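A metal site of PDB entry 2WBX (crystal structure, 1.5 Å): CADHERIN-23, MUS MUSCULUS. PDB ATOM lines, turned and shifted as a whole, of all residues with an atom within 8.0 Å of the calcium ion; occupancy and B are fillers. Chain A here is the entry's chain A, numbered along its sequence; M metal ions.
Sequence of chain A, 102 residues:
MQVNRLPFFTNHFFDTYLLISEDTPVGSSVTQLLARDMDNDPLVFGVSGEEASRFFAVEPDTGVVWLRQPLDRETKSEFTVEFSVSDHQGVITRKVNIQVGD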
ATOM      1  N   VAL A   3      -2.490  -0.745 -22.084  1.00  0.00           N
ATOM      2  CA  VAL A   3      -2.826  -2.137 -22.282  1.00  0.00           C
ATOM      3  C   VAL A   3      -1.970  -2.657 -23.420  1.00  0.00           C
ATOM      4  O   VAL A   3      -2.190  -2.294 -24.597  1.00  0.00           O
ATOM      5  CB  VAL A   3      -4.329  -2.309 -22.571  1.00  0.00           C
ATOM      6  CG1 VAL A   3      -4.636  -3.793 -22.778  1.00  0.00           C
ATOM      7  CG2 VAL A   3      -5.166  -1.721 -21.419  1.00  0.00           C
ATOM      8  N   ASN A   4      -0.962  -3.451 -23.073  1.00  0.00           N
ATOM      9  CA  ASN A   4      -0.012  -3.922 -24.089  1.00  0.00           C
ATOM     10  C   ASN A   4       0.682  -5.159 -23.629  1.00  0.00           C
ATOM     11  O   ASN A   4       1.050  -5.292 -22.458  1.00  0.00           O
ATOM     12  CB  ASN A   4       1.031  -2.860 -24.427  1.00  0.00           C
ATOM     13  CG  ASN A   4       1.921  -3.298 -25.588  1.00  0.00           C
ATOM     14  OD1 ASN A   4       1.431  -3.645 -26.620  1.00  0.00           O
ATOM     15  ND2 ASN A   4       3.214  -3.320 -25.392  1.00  0.00           N
ATOM     16  N   ARG A   5       0.847  -6.072 -24.575  1.00  0.00           N
ATOM     17  CA  ARG A   5       1.704  -7.212 -24.377  1.00  0.00           C
ATOM     18  C   ARG A   5       2.852  -7.120 -25.350  1.00  0.00           C
ATOM     19  O   ARG A   5       2.681  -6.705 -26.495  1.00  0.00           O
ATOM     20  CB  ARG A   5       0.897  -8.461 -24.570  1.00  0.00           C
ATOM     21  CG  ARG A   5      -0.058  -8.555 -23.375  1.00  0.00           C
ATOM     22  CD  ARG A   5      -1.356  -9.158 -23.640  1.00  0.00           C
ATOM     23  NE  ARG A   5      -2.152  -8.567 -24.700  1.00  0.00           N
ATOM     24  CZ  ARG A   5      -3.237  -9.167 -25.179  1.00  0.00           C
ATOM     25  NH1 ARG A   5      -3.930  -8.620 -26.150  1.00  0.00           N
ATOM     26  NH2 ARG A   5      -3.590 -10.333 -24.652  1.00  0.00           N
ATOM     27  N   LEU A   6       4.038  -7.461 -24.881  1.00  0.00           N
ATOM     28  CA  LEU A   6       5.200  -7.418 -25.734  1.00  0.00           C
ATOM     29  C   LEU A   6       5.178  -8.593 -26.707  1.00  0.00           C
ATOM     30  O   LEU A   6       4.635  -9.648 -26.417  1.00  0.00           O
ATOM     31  CB  LEU A   6       6.491  -7.395 -24.944  1.00  0.00           C
ATOM     32  CG  LEU A   6       6.755  -6.139 -24.073  1.00  0.00           C
ATOM     33  CD1 LEU A   6       8.147  -6.190 -23.423  1.00  0.00           C
ATOM     34  CD2 LEU A   6       6.656  -4.876 -24.871  1.00  0.00           C
ATOM     35  N   PRO A   7       5.802  -8.410 -27.872  1.00  0.00           N
ATOM     36  CA  PRO A   7       5.868  -9.510 -28.839  1.00  0.00           C
ATOM     37  C   PRO A   7       6.839 -10.584 -28.346  1.00  0.00           C
ATOM     38  O   PRO A   7       7.639 -10.367 -27.419  1.00  0.00           O
ATOM     39  CB  PRO A   7       6.391  -8.819 -30.087  1.00  0.00           C
ATOM     40  CG  PRO A   7       7.205  -7.645 -29.540  1.00  0.00           C
ATOM     41  CD  PRO A   7       6.385  -7.160 -28.415  1.00  0.00           C
ATOM     42  N   ARG A  36       4.990 -13.048 -32.764  1.00  0.00           N
ATOM     43  CA  ARG A  36       3.585 -12.756 -32.530  1.00  0.00           C
ATOM     44  C   ARG A  36       3.446 -11.662 -31.484  1.00  0.00           C
ATOM     45  O   ARG A  36       4.149 -11.647 -30.491  1.00  0.00           O
ATOM     46  CB  ARG A  36       2.821 -14.005 -32.136  1.00  0.00           C
ATOM     47  CG  ARG A  36       1.353 -13.908 -32.448  1.00  0.00           C
ATOM     48  CD  ARG A  36       0.561 -13.508 -31.239  1.00  0.00           C
ATOM     49  NE  ARG A  36      -0.850 -13.266 -31.518  1.00  0.00           N
ATOM     50  CZ  ARG A  36      -1.781 -14.216 -31.596  1.00  0.00           C
ATOM     51  NH1 ARG A  36      -1.466 -15.493 -31.422  1.00  0.00           N
ATOM     52  NH2 ARG A  36      -3.036 -13.878 -31.852  1.00  0.00           N
ATOM     53  N   ASP A  37       2.573 -10.722 -31.756  1.00  0.00           N
ATOM     54  CA  ASP A  37       2.166  -9.708 -30.799  1.00  0.00           C
ATOM     55  C   ASP A  37       0.687  -9.986 -30.489  1.00  0.00           C
ATOM     56  O   ASP A  37      -0.161  -9.926 -31.397  1.00  0.00           O
ATOM     57  CB  ASP A  37       2.344  -8.322 -31.347  1.00  0.00           C
ATOM     58  CG  ASP A  37       2.121  -7.253 -30.299  1.00  0.00           C
ATOM     59  OD1 ASP A  37       3.090  -6.683 -29.770  1.00  0.00           O
ATOM     60  OD2 ASP A  37       0.942  -6.965 -29.982  1.00  0.00           O
ATOM     61  N   MET A  38       0.365 -10.285 -29.231  1.00  0.00           N
ATOM     62  CA  MET A  38      -1.017 -10.645 -28.893  1.00  0.00           C
ATOM     63  C   MET A  38      -2.018  -9.532 -29.082  1.00  0.00           C
ATOM     64  O   MET A  38      -3.216  -9.801 -29.074  1.00  0.00           O
ATOM     65  CB  MET A  38      -1.104 -11.196 -27.468  1.00  0.00           C
ATOM     66  CG  MET A  38      -0.337 -12.485 -27.255  1.00  0.00           C
ATOM     67  SD  MET A  38      -0.776 -13.852 -28.355  1.00  0.00           S
ATOM     68  CE  MET A  38      -2.502 -13.656 -28.322  1.00  0.00           C
ATOM     69  N   ASP A  39      -1.535  -8.292 -29.174  1.00  0.00           N
ATOM     70  CA  ASP A  39      -2.381  -7.139 -29.465  1.00  0.00           C
ATOM     71  C   ASP A  39      -2.515  -6.876 -30.960  1.00  0.00           C
ATOM     72  O   ASP A  39      -3.219  -5.945 -31.372  1.00  0.00           O
ATOM     73  CB  ASP A  39      -1.833  -5.862 -28.783  1.00  0.00           C
ATOM     74  CG  ASP A  39      -1.381  -6.104 -27.380  1.00  0.00           C
ATOM     75  OD1 ASP A  39      -2.251  -6.427 -26.527  1.00  0.00           O
ATOM     76  OD2 ASP A  39      -0.148  -5.949 -27.156  1.00  0.00           O
ATOM     77  N   ASN A  40      -1.857  -7.700 -31.789  1.00  0.00           N
ATOM     78  CA  ASN A  40      -1.775  -7.479 -33.239  1.00  0.00           C
ATOM     79  C   ASN A  40      -1.061  -6.165 -33.596  1.00  0.00           C
ATOM     80  O   ASN A  40      -1.284  -5.614 -34.669  1.00  0.00           O
ATOM     81  CB  ASN A  40      -3.156  -7.501 -33.907  1.00  0.00           C
ATOM     82  CG  ASN A  40      -3.954  -8.692 -33.519  1.00  0.00           C
ATOM     83  OD1 ASN A  40      -3.439  -9.818 -33.492  1.00  0.00           O
ATOM     84  ND2 ASN A  40      -5.238  -8.472 -33.244  1.00  0.00           N
ATOM     85  N   ASP A  41      -0.207  -5.674 -32.700  1.00  0.00           N
ATOM     86  CA  ASP A  41       0.553  -4.460 -32.997  1.00  0.00           C
ATOM     87  C   ASP A  41       1.557  -4.703 -34.110  1.00  0.00           C
ATOM     88  O   ASP A  41       2.154  -5.795 -34.183  1.00  0.00           O
ATOM     89  CB  ASP A  41       1.291  -3.988 -31.757  1.00  0.00           C
ATOM     90  CG  ASP A  41       0.384  -3.498 -30.646  1.00  0.00           C
ATOM     91  OD1 ASP A  41      -0.658  -2.876 -30.941  1.00  0.00           O
ATOM     92  OD2 ASP A  41       0.748  -3.683 -29.449  1.00  0.00           O
ATOM     93  N   PRO A  42       1.792  -3.701 -34.970  1.00  0.00           N
ATOM     94  CA  PRO A  42       2.861  -3.786 -35.961  1.00  0.00           C
ATOM     95  C   PRO A  42       4.218  -4.006 -35.292  1.00  0.00           C
ATOM     96  O   PRO A  42       4.530  -3.397 -34.271  1.00  0.00           O
ATOM     97  CB  PRO A  42       2.824  -2.428 -36.669  1.00  0.00           C
ATOM     98  CG  PRO A  42       1.481  -1.900 -36.376  1.00  0.00           C
ATOM     99  CD  PRO A  42       0.991  -2.490 -35.114  1.00  0.00           C
ATOM    100  N   LEU A  43       5.007  -4.869 -35.899  1.00  0.00           N
ATOM    101  CA  LEU A  43       6.297  -5.263 -35.320  1.00  0.00           C
ATOM    102  C   LEU A  43       7.469  -4.878 -36.217  1.00  0.00           C
ATOM    103  O   LEU A  43       7.363  -4.881 -37.460  1.00  0.00           O
ATOM    104  CB  LEU A  43       6.328  -6.767 -35.109  1.00  0.00           C
ATOM    105  CG  LEU A  43       5.306  -7.330 -34.126  1.00  0.00           C
ATOM    106  CD1 LEU A  43       5.529  -8.822 -34.015  1.00  0.00           C
ATOM    107  CD2 LEU A  43       5.384  -6.604 -32.769  1.00  0.00           C
ATOM    108  N   SER A  86      10.241  -5.728 -31.790  1.00  0.00           N
ATOM    109  CA  SER A  86       9.639  -4.649 -31.030  1.00  0.00           C
ATOM    110  C   SER A  86       8.253  -4.272 -31.509  1.00  0.00           C
ATOM    111  O   SER A  86       8.014  -4.257 -32.719  1.00  0.00           O
ATOM    112  CB  SER A  86      10.546  -3.422 -31.170  1.00  0.00           C
ATOM    113  OG  SER A  86      10.017  -2.296 -30.550  1.00  0.00           O
ATOM    114  N   ASP A  87       7.408  -3.838 -30.573  1.00  0.00           N
ATOM    115  CA  ASP A  87       6.130  -3.234 -30.915  1.00  0.00           C
ATOM    116  C   ASP A  87       6.149  -1.735 -30.680  1.00  0.00           C
ATOM    117  O   ASP A  87       5.092  -1.116 -30.643  1.00  0.00           O
ATOM    118  CB  ASP A  87       4.922  -3.888 -30.187  1.00  0.00           C
ATOM    119  CG  ASP A  87       4.958  -3.716 -28.699  1.00  0.00           C
ATOM    120  OD1 ASP A  87       5.874  -3.056 -28.161  1.00  0.00           O
ATOM    121  OD2 ASP A  87       4.003  -4.216 -28.029  1.00  0.00           O
ATOM    122  N   HIS A  88       7.352  -1.176 -30.524  1.00  0.00           N
ATOM    123  CA  HIS A  88       7.554   0.247 -30.267  1.00  0.00           C
ATOM    124  C   HIS A  88       7.282   0.660 -28.800  1.00  0.00           C
ATOM    125  O   HIS A  88       7.566   1.801 -28.432  1.00  0.00           O
ATOM    126  CB  HIS A  88       6.781   1.140 -31.271  1.00  0.00           C
ATOM    127  CG  HIS A  88       7.040   0.793 -32.708  1.00  0.00           C
ATOM    128  ND1 HIS A  88       8.260   0.970 -33.318  1.00  0.00           N
ATOM    129  CD2 HIS A  88       6.218   0.300 -33.665  1.00  0.00           C
ATOM    130  CE1 HIS A  88       8.190   0.583 -34.582  1.00  0.00           C
ATOM    131  NE2 HIS A  88       6.949   0.192 -34.823  1.00  0.00           N
ATOM    132  N   GLN A  89       6.714  -0.232 -27.984  1.00  0.00           N
ATOM    133  CA  GLN A  89       6.566  -0.025 -26.536  1.00  0.00           C
ATOM    134  C   GLN A  89       7.675  -0.793 -25.794  1.00  0.00           C
ATOM    135  O   GLN A  89       8.225  -0.372 -24.765  1.00  0.00           O
ATOM    136  CB  GLN A  89       5.152  -0.478 -26.121  1.00  0.00           C
ATOM    137  CG  GLN A  89       4.056   0.417 -26.767  1.00  0.00           C
ATOM    138  CD  GLN A  89       2.837  -0.301 -27.406  1.00  0.00           C
ATOM    139  OE1 GLN A  89       1.709  -0.214 -26.893  1.00  0.00           O
ATOM    140  NE2 GLN A  89       3.041  -0.959 -28.549  1.00  0.00           N
ATOM    141  N   GLY A  90       7.994  -1.956 -26.310  1.00  0.00           N
ATOM    142  CA  GLY A  90       9.045  -2.762 -25.749  1.00  0.00           C
ATOM    143  C   GLY A  90       9.732  -3.602 -26.798  1.00  0.00           C
ATOM    144  O   GLY A  90       9.214  -3.770 -27.896  1.00  0.00           O
HETATM  145 CA    CA M   1       1.874  -5.295 -28.208  1.00  0.00          CA
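The calcium ion is bound by OD2 of Asp 41 (2.3 Å), OD1 of Asn 4 (2.3 Å), O of Arg 5 (2.4 Å), OD2 of Asp 39 (2.4 Å), OD2 of Asp 87 (2.4 Å), OD1 of Asp 37 (2.4 Å) and OD2 of Asp 37 (2.6 Å). The calcium ion has seven donor atoms within binding distance.
OE1 of Gln 89 sits close to OD1 of Asn 4. NH1 of Arg 5 lies within hydrogen-bond range of O of Met 38 (3.2 Å). O of Asp 87 lies within hydrogen-bond range of NE2 of Gln 89 (2.9 Å). The backbone NH (N) of Gly 90 lies within hydrogen-bond range of the side-chain carboxylate (OD1) of Asp 87, 3.0 Å away. OD2 of Asp 37 sits close to N of Asn 40 (3.4 Å).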
